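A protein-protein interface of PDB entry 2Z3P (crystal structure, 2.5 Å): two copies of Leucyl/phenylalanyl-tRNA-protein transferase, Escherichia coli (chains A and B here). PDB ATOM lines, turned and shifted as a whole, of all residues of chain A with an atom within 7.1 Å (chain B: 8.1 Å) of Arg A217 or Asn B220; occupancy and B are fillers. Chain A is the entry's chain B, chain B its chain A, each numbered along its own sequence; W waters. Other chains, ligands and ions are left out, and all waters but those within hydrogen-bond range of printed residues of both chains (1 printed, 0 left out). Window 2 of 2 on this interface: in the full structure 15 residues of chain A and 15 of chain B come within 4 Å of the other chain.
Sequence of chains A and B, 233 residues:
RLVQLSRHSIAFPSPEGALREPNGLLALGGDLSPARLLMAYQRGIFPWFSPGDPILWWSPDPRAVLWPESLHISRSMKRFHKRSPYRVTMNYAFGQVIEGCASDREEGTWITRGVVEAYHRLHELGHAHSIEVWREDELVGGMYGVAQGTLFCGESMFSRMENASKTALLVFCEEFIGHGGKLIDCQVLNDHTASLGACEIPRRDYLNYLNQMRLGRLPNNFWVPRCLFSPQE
O of Leu B125 lies close to ND2 of Asn A220 (3.4 Å). O of Leu A215 is in hydrogen-bond range of ND2 of Asn B221, at 2.8 Å. The backbone carbonyl oxygen (O) of Asn B220 is in hydrogen-bond range of the guanidinium group (NH1) of Arg A217.
The guanidinium group (NH2) of Arg A217 is in hydrogen-bond range of the side-chain amide oxygen (OD1) of Asn A220, 2.7 Å away.
Among the printed residues, pairs that only touch across the chains: Leu A215 with Val B224 (3.9 Å), Gly A216 with Val B224 (3.7 Å) and Arg A217 with Val B224 (3.7 Å).
Of the printed residues of chain B, Leu A215 touches Asn B221 (2.8 Å) and Val B224 (3.9 Å). Gly A216 touches one residue of chain B. Of chain B, only Asn B220 (2.9 Å) and Val B224 (3.7 Å) come within 4 Å of Arg A217. Of the printed residues of chain A, Leu B125 touches Asn A220. Of the printed residues of chain A, Asn B220 touches Arg A217 (2.9 Å). Printed residues of chain A within 4 Å of Asn B221: Leu A215 (2.8 Å). Trp B223 touches none of the printed residues of chain A. Printed residues of chain A within 4 Å of Val B224: Leu A215, Gly A216 and Arg A217. The nearest residue of chain B that does not touch Arg A217 is Asn B221 (4.1 Å). The nearest residue of chain A that does not touch Asn B220 is Leu A215 (6.6 Å).
Hydrophobic or aromatic side chains of chain A that line the printed part of chain B: Leu A215. Printed residues of chain B that touch a printed residue of chain A: Leu B125, Asn B220, Asn B221 and Val B224. Hydrophobic or aromatic side chains of chain B that line the printed part of chain A: Val B224. Among the printed residues, 6 pairs touch across the chains. Among the printed residues, no Asp or Glu carboxylate lies within 4 Å of a Lys or Arg side-chain nitrogen of the other chain.
Arg A217 touches Asn B220, but with the chains exchanged Asn A220 does not touch Arg B217 (9.0 Å). Of the 6 pairs that touch across the chains among the printed residues, none has its exchanged pair printed and touching as well.
Water W1 bridges O of Arg A214 and O of Pro B225.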
ATOM      1  N   GLY A 149      14.814  20.408 -29.284  1.00  0.00           N
ATOM      2  CA  GLY A 149      15.760  20.678 -28.222  1.00  0.00           C
ATOM      3  C   GLY A 149      16.692  21.824 -28.559  1.00  0.00           C
ATOM      4  O   GLY A 149      16.259  22.962 -28.708  1.00  0.00           O
ATOM      5  N   THR A 150      17.979  21.519 -28.663  1.00  0.00           N
ATOM      6  CA  THR A 150      19.003  22.501 -28.987  1.00  0.00           C
ATOM      7  C   THR A 150      19.338  22.312 -30.454  1.00  0.00           C
ATOM      8  O   THR A 150      20.277  22.917 -30.976  1.00  0.00           O
ATOM      9  CB  THR A 150      20.275  22.253 -28.173  1.00  0.00           C
ATOM     10  OG1 THR A 150      20.729  20.913 -28.411  1.00  0.00           O
ATOM     11  CG2 THR A 150      20.008  22.426 -26.704  1.00  0.00           C
ATOM     12  N   HIS A 179      22.276  31.474 -27.207  1.00  0.00           N
ATOM     13  CA  HIS A 179      21.454  30.911 -26.144  1.00  0.00           C
ATOM     14  C   HIS A 179      21.451  29.394 -26.004  1.00  0.00           C
ATOM     15  O   HIS A 179      20.523  28.829 -25.435  1.00  0.00           O
ATOM     16  CB  HIS A 179      20.019  31.413 -26.278  1.00  0.00           C
ATOM     17  CG  HIS A 179      19.852  32.839 -25.863  1.00  0.00           C
ATOM     18  ND1 HIS A 179      19.472  33.832 -26.740  1.00  0.00           N
ATOM     19  CD2 HIS A 179      20.054  33.447 -24.669  1.00  0.00           C
ATOM     20  CE1 HIS A 179      19.450  34.991 -26.106  1.00  0.00           C
ATOM     21  NE2 HIS A 179      19.801  34.785 -24.849  1.00  0.00           N
ATOM     22  N   GLY A 180      22.479  28.735 -26.518  1.00  0.00           N
ATOM     23  CA  GLY A 180      22.548  27.296 -26.371  1.00  0.00           C
ATOM     24  C   GLY A 180      22.421  26.449 -27.616  1.00  0.00           C
ATOM     25  O   GLY A 180      22.838  25.289 -27.598  1.00  0.00           O
ATOM     26  N   GLY A 181      21.850  26.998 -28.687  1.00  0.00           N
ATOM     27  CA  GLY A 181      21.692  26.221 -29.906  1.00  0.00           C
ATOM     28  C   GLY A 181      22.970  25.511 -30.314  1.00  0.00           C
ATOM     29  O   GLY A 181      24.060  26.057 -30.165  1.00  0.00           O
ATOM     30  N   MET A 213      20.596  16.057 -28.493  1.00  0.00           N
ATOM     31  CA  MET A 213      20.146  17.445 -28.381  1.00  0.00           C
ATOM     32  C   MET A 213      18.647  17.669 -28.188  1.00  0.00           C
ATOM     33  O   MET A 213      18.227  18.756 -27.766  1.00  0.00           O
ATOM     34  CB  MET A 213      20.605  18.228 -29.613  1.00  0.00           C
ATOM     35  CG  MET A 213      22.096  18.231 -29.796  1.00  0.00           C
ATOM     36  SD  MET A 213      22.611  19.132 -31.255  1.00  0.00           S
ATOM     37  CE  MET A 213      23.587  17.923 -32.067  1.00  0.00           C
ATOM     38  N   ARG A 214      17.832  16.665 -28.496  1.00  0.00           N
ATOM     39  CA  ARG A 214      16.398  16.842 -28.335  1.00  0.00           C
ATOM     40  C   ARG A 214      15.956  16.936 -26.869  1.00  0.00           C
ATOM     41  O   ARG A 214      14.885  17.462 -26.579  1.00  0.00           O
ATOM     42  CB  ARG A 214      15.631  15.730 -29.061  1.00  0.00           C
ATOM     43  CG  ARG A 214      15.729  14.349 -28.465  1.00  0.00           C
ATOM     44  CD  ARG A 214      14.827  13.398 -29.245  1.00  0.00           C
ATOM     45  NE  ARG A 214      14.149  12.444 -28.375  1.00  0.00           N
ATOM     46  CZ  ARG A 214      14.732  11.387 -27.826  1.00  0.00           C
ATOM     47  NH1 ARG A 214      16.014  11.133 -28.060  1.00  0.00           N
ATOM     48  NH2 ARG A 214      14.036  10.591 -27.025  1.00  0.00           N
ATOM     49  N   LEU A 215      16.779  16.452 -25.943  1.00  0.00           N
ATOM     50  CA  LEU A 215      16.427  16.520 -24.519  1.00  0.00           C
ATOM     51  C   LEU A 215      17.068  17.715 -23.829  1.00  0.00           C
ATOM     52  O   LEU A 215      16.932  17.904 -22.618  1.00  0.00           O
ATOM     53  CB  LEU A 215      16.826  15.235 -23.805  1.00  0.00           C
ATOM     54  CG  LEU A 215      16.174  13.995 -24.413  1.00  0.00           C
ATOM     55  CD1 LEU A 215      16.804  12.743 -23.822  1.00  0.00           C
ATOM     56  CD2 LEU A 215      14.658  14.054 -24.175  1.00  0.00           C
ATOM     57  N   GLY A 216      17.777  18.518 -24.615  1.00  0.00           N
ATOM     58  CA  GLY A 216      18.397  19.711 -24.081  1.00  0.00           C
ATOM     59  C   GLY A 216      17.355  20.804 -24.165  1.00  0.00           C
ATOM     60  O   GLY A 216      16.222  20.549 -24.564  1.00  0.00           O
ATOM     61  N   ARG A 217      17.718  22.022 -23.799  1.00  0.00           N
ATOM     62  CA  ARG A 217      16.757  23.104 -23.855  1.00  0.00           C
ATOM     63  C   ARG A 217      17.411  24.466 -23.975  1.00  0.00           C
ATOM     64  O   ARG A 217      18.604  24.619 -23.726  1.00  0.00           O
ATOM     65  CB  ARG A 217      15.856  23.065 -22.619  1.00  0.00           C
ATOM     66  CG  ARG A 217      16.608  22.924 -21.310  1.00  0.00           C
ATOM     67  CD  ARG A 217      15.707  23.181 -20.113  1.00  0.00           C
ATOM     68  NE  ARG A 217      15.127  24.517 -20.154  1.00  0.00           N
ATOM     69  CZ  ARG A 217      14.695  25.180 -19.085  1.00  0.00           C
ATOM     70  NH1 ARG A 217      14.780  24.628 -17.883  1.00  0.00           N
ATOM     71  NH2 ARG A 217      14.177  26.396 -19.216  1.00  0.00           N
ATOM     72  N   LEU A 218      16.600  25.443 -24.373  1.00  0.00           N
ATOM     73  CA  LEU A 218      17.017  26.830 -24.536  1.00  0.00           C
ATOM     74  C   LEU A 218      16.191  27.614 -23.517  1.00  0.00           C
ATOM     75  O   LEU A 218      15.256  27.073 -22.931  1.00  0.00           O
ATOM     76  CB  LEU A 218      16.694  27.300 -25.957  1.00  0.00           C
ATOM     77  CG  LEU A 218      17.264  26.465 -27.114  1.00  0.00           C
ATOM     78  CD1 LEU A 218      16.584  26.845 -28.415  1.00  0.00           C
ATOM     79  CD2 LEU A 218      18.775  26.679 -27.218  1.00  0.00           C
ATOM     80  N   PRO A 219      16.522  28.894 -23.285  1.00  0.00           N
ATOM     81  CA  PRO A 219      15.745  29.669 -22.313  1.00  0.00           C
ATOM     82  C   PRO A 219      14.252  29.482 -22.550  1.00  0.00           C
ATOM     83  O   PRO A 219      13.827  29.339 -23.691  1.00  0.00           O
ATOM     84  CB  PRO A 219      16.187  31.103 -22.586  1.00  0.00           C
ATOM     85  CG  PRO A 219      17.606  30.932 -23.007  1.00  0.00           C
ATOM     86  CD  PRO A 219      17.531  29.746 -23.939  1.00  0.00           C
ATOM     87  N   ASN A 220      13.468  29.486 -21.475  1.00  0.00           N
ATOM     88  CA  ASN A 220      12.022  29.316 -21.569  1.00  0.00           C
ATOM     89  C   ASN A 220      11.349  30.243 -22.573  1.00  0.00           C
ATOM     90  O   ASN A 220      10.337  29.892 -23.177  1.00  0.00           O
ATOM     91  CB  ASN A 220      11.367  29.539 -20.203  1.00  0.00           C
ATOM     92  CG  ASN A 220      11.449  28.321 -19.309  1.00  0.00           C
ATOM     93  OD1 ASN A 220      11.641  27.196 -19.782  1.00  0.00           O
ATOM     94  ND2 ASN A 220      11.280  28.534 -18.006  1.00  0.00           N
ATOM     95  N   ASN A 221      11.916  31.426 -22.752  1.00  0.00           N
ATOM     96  CA  ASN A 221      11.337  32.402 -23.656  1.00  0.00           C
ATOM     97  C   ASN A 221      12.025  32.505 -25.003  1.00  0.00           C
ATOM     98  O   ASN A 221      11.741  33.422 -25.772  1.00  0.00           O
ATOM     99  CB  ASN A 221      11.320  33.768 -22.975  1.00  0.00           C
ATOM    100  CG  ASN A 221      12.674  34.150 -22.416  1.00  0.00           C
ATOM    101  OD1 ASN A 221      12.776  35.014 -21.542  1.00  0.00           O
ATOM    102  ND2 ASN A 221      13.728  33.513 -22.923  1.00  0.00           N
ATOM    103  N   LEU B 125       5.637  30.352 -21.515  1.00  0.00           N
ATOM    104  CA  LEU B 125       6.667  30.769 -20.573  1.00  0.00           C
ATOM    105  C   LEU B 125       7.348  29.629 -19.816  1.00  0.00           C
ATOM    106  O   LEU B 125       8.331  29.858 -19.109  1.00  0.00           O
ATOM    107  CB  LEU B 125       6.081  31.771 -19.576  1.00  0.00           C
ATOM    108  CG  LEU B 125       5.638  33.099 -20.203  1.00  0.00           C
ATOM    109  CD1 LEU B 125       4.873  33.940 -19.180  1.00  0.00           C
ATOM    110  CD2 LEU B 125       6.863  33.847 -20.720  1.00  0.00           C
ATOM    111  N   GLY B 126       6.832  28.411 -19.941  1.00  0.00           N
ATOM    112  CA  GLY B 126       7.466  27.288 -19.266  1.00  0.00           C
ATOM    113  C   GLY B 126       7.031  26.950 -17.847  1.00  0.00           C
ATOM    114  O   GLY B 126       7.728  26.214 -17.145  1.00  0.00           O
ATOM    115  N   HIS B 179      12.269  11.700 -10.433  1.00  0.00           N
ATOM    116  CA  HIS B 179      13.182  12.834 -10.481  1.00  0.00           C
ATOM    117  C   HIS B 179      13.027  13.895  -9.408  1.00  0.00           C
ATOM    118  O   HIS B 179      13.446  15.029  -9.616  1.00  0.00           O
ATOM    119  CB  HIS B 179      13.119  13.505 -11.847  1.00  0.00           C
ATOM    120  CG  HIS B 179      13.522  12.611 -12.977  1.00  0.00           C
ATOM    121  ND1 HIS B 179      12.718  11.593 -13.445  1.00  0.00           N
ATOM    122  CD2 HIS B 179      14.633  12.595 -13.748  1.00  0.00           C
ATOM    123  CE1 HIS B 179      13.313  10.994 -14.461  1.00  0.00           C
ATOM    124  NE2 HIS B 179      14.478  11.583 -14.664  1.00  0.00           N
ATOM    125  N   ARG B 217      13.717  21.567  -6.550  1.00  0.00           N
ATOM    126  CA  ARG B 217      14.003  21.617  -7.972  1.00  0.00           C
ATOM    127  C   ARG B 217      14.062  20.235  -8.627  1.00  0.00           C
ATOM    128  O   ARG B 217      14.481  19.253  -8.012  1.00  0.00           O
ATOM    129  CB  ARG B 217      15.320  22.365  -8.179  1.00  0.00           C
ATOM    130  CG  ARG B 217      15.280  23.396  -9.278  1.00  0.00           C
ATOM    131  CD  ARG B 217      16.306  24.484  -9.035  1.00  0.00           C
ATOM    132  NE  ARG B 217      16.337  25.458 -10.125  1.00  0.00           N
ATOM    133  CZ  ARG B 217      16.901  26.659 -10.039  1.00  0.00           C
ATOM    134  NH1 ARG B 217      17.484  27.040  -8.909  1.00  0.00           N
ATOM    135  NH2 ARG B 217      16.885  27.480 -11.082  1.00  0.00           N
ATOM    136  N   LEU B 218      13.620  20.173  -9.879  1.00  0.00           N
ATOM    137  CA  LEU B 218      13.610  18.938 -10.655  1.00  0.00           C
ATOM    138  C   LEU B 218      14.715  19.084 -11.688  1.00  0.00           C
ATOM    139  O   LEU B 218      15.278  20.164 -11.833  1.00  0.00           O
ATOM    140  CB  LEU B 218      12.262  18.778 -11.363  1.00  0.00           C
ATOM    141  CG  LEU B 218      11.018  18.572 -10.491  1.00  0.00           C
ATOM    142  CD1 LEU B 218       9.765  18.707 -11.340  1.00  0.00           C
ATOM    143  CD2 LEU B 218      11.071  17.187  -9.826  1.00  0.00           C
ATOM    144  N   PRO B 219      15.050  18.004 -12.413  1.00  0.00           N
ATOM    145  CA  PRO B 219      16.111  18.126 -13.414  1.00  0.00           C
ATOM    146  C   PRO B 219      15.834  19.312 -14.329  1.00  0.00           C
ATOM    147  O   PRO B 219      14.689  19.590 -14.682  1.00  0.00           O
ATOM    148  CB  PRO B 219      16.043  16.790 -14.152  1.00  0.00           C
ATOM    149  CG  PRO B 219      15.650  15.843 -13.070  1.00  0.00           C
ATOM    150  CD  PRO B 219      14.560  16.615 -12.336  1.00  0.00           C
ATOM    151  N   ASN B 220      16.893  20.004 -14.716  1.00  0.00           N
ATOM    152  CA  ASN B 220      16.757  21.172 -15.569  1.00  0.00           C
ATOM    153  C   ASN B 220      15.963  20.938 -16.848  1.00  0.00           C
ATOM    154  O   ASN B 220      15.347  21.864 -17.366  1.00  0.00           O
ATOM    155  CB  ASN B 220      18.140  21.723 -15.925  1.00  0.00           C
ATOM    156  CG  ASN B 220      18.062  23.061 -16.628  1.00  0.00           C
ATOM    157  OD1 ASN B 220      17.645  23.148 -17.781  1.00  0.00           O
ATOM    158  ND2 ASN B 220      18.454  24.121 -15.927  1.00  0.00           N
ATOM    159  N   ASN B 221      15.963  19.712 -17.356  1.00  0.00           N
ATOM    160  CA  ASN B 221      15.251  19.418 -18.595  1.00  0.00           C
ATOM    161  C   ASN B 221      14.038  18.502 -18.414  1.00  0.00           C
ATOM    162  O   ASN B 221      13.553  17.928 -19.385  1.00  0.00           O
ATOM    163  CB  ASN B 221      16.212  18.776 -19.581  1.00  0.00           C
ATOM    164  CG  ASN B 221      16.589  17.386 -19.167  1.00  0.00           C
ATOM    165  OD1 ASN B 221      16.672  17.096 -17.967  1.00  0.00           O
ATOM    166  ND2 ASN B 221      16.819  16.507 -20.145  1.00  0.00           N
ATOM    167  N   PHE B 222      13.550  18.381 -17.183  1.00  0.00           N
ATOM    168  CA  PHE B 222      12.402  17.522 -16.872  1.00  0.00           C
ATOM    169  C   PHE B 222      11.169  17.741 -17.748  1.00  0.00           C
ATOM    170  O   PHE B 222      10.517  16.782 -18.156  1.00  0.00           O
ATOM    171  CB  PHE B 222      11.988  17.695 -15.405  1.00  0.00           C
ATOM    172  CG  PHE B 222      10.895  16.753 -14.963  1.00  0.00           C
ATOM    173  CD1 PHE B 222      11.164  15.403 -14.745  1.00  0.00           C
ATOM    174  CD2 PHE B 222       9.585  17.205 -14.817  1.00  0.00           C
ATOM    175  CE1 PHE B 222      10.143  14.519 -14.392  1.00  0.00           C
ATOM    176  CE2 PHE B 222       8.557  16.332 -14.466  1.00  0.00           C
ATOM    177  CZ  PHE B 222       8.835  14.984 -14.254  1.00  0.00           C
ATOM    178  N   TRP B 223      10.871  19.000 -18.048  1.00  0.00           N
ATOM    179  CA  TRP B 223       9.695  19.352 -18.829  1.00  0.00           C
ATOM    180  C   TRP B 223       9.812  19.497 -20.359  1.00  0.00           C
ATOM    181  O   TRP B 223       8.807  19.730 -21.033  1.00  0.00           O
ATOM    182  CB  TRP B 223       9.088  20.626 -18.256  1.00  0.00           C
ATOM    183  CG  TRP B 223       8.743  20.540 -16.785  1.00  0.00           C
ATOM    184  CD1 TRP B 223       9.449  21.078 -15.742  1.00  0.00           C
ATOM    185  CD2 TRP B 223       7.585  19.909 -16.201  1.00  0.00           C
ATOM    186  NE1 TRP B 223       8.800  20.825 -14.548  1.00  0.00           N
ATOM    187  CE2 TRP B 223       7.658  20.112 -14.802  1.00  0.00           C
ATOM    188  CE3 TRP B 223       6.500  19.193 -16.727  1.00  0.00           C
ATOM    189  CZ2 TRP B 223       6.684  19.629 -13.923  1.00  0.00           C
ATOM    190  CZ3 TRP B 223       5.529  18.712 -15.853  1.00  0.00           C
ATOM    191  CH2 TRP B 223       5.627  18.932 -14.467  1.00  0.00           C
ATOM    192  N   VAL B 224      11.006  19.370 -20.923  1.00  0.00           N
ATOM    193  CA  VAL B 224      11.124  19.501 -22.375  1.00  0.00           C
ATOM    194  C   VAL B 224      10.209  18.446 -23.010  1.00  0.00           C
ATOM    195  O   VAL B 224      10.010  17.368 -22.452  1.00  0.00           O
ATOM    196  CB  VAL B 224      12.598  19.292 -22.863  1.00  0.00           C
ATOM    197  CG1 VAL B 224      13.542  20.209 -22.084  1.00  0.00           C
ATOM    198  CG2 VAL B 224      13.024  17.834 -22.686  1.00  0.00           C
ATOM    199  N   PRO B 225       9.619  18.754 -24.174  1.00  0.00           N
ATOM    200  CA  PRO B 225       8.732  17.779 -24.821  1.00  0.00           C
ATOM    201  C   PRO B 225       9.421  16.457 -25.090  1.00  0.00           C
ATOM    202  O   PRO B 225      10.545  16.429 -25.575  1.00  0.00           O
ATOM    203  CB  PRO B 225       8.294  18.494 -26.101  1.00  0.00           C
ATOM    204  CG  PRO B 225       9.386  19.512 -26.331  1.00  0.00           C
ATOM    205  CD  PRO B 225       9.683  20.003 -24.944  1.00  0.00           C
HETATM  206  O   HOH W   1      12.365  18.479 -27.210  1.00  0.00           O
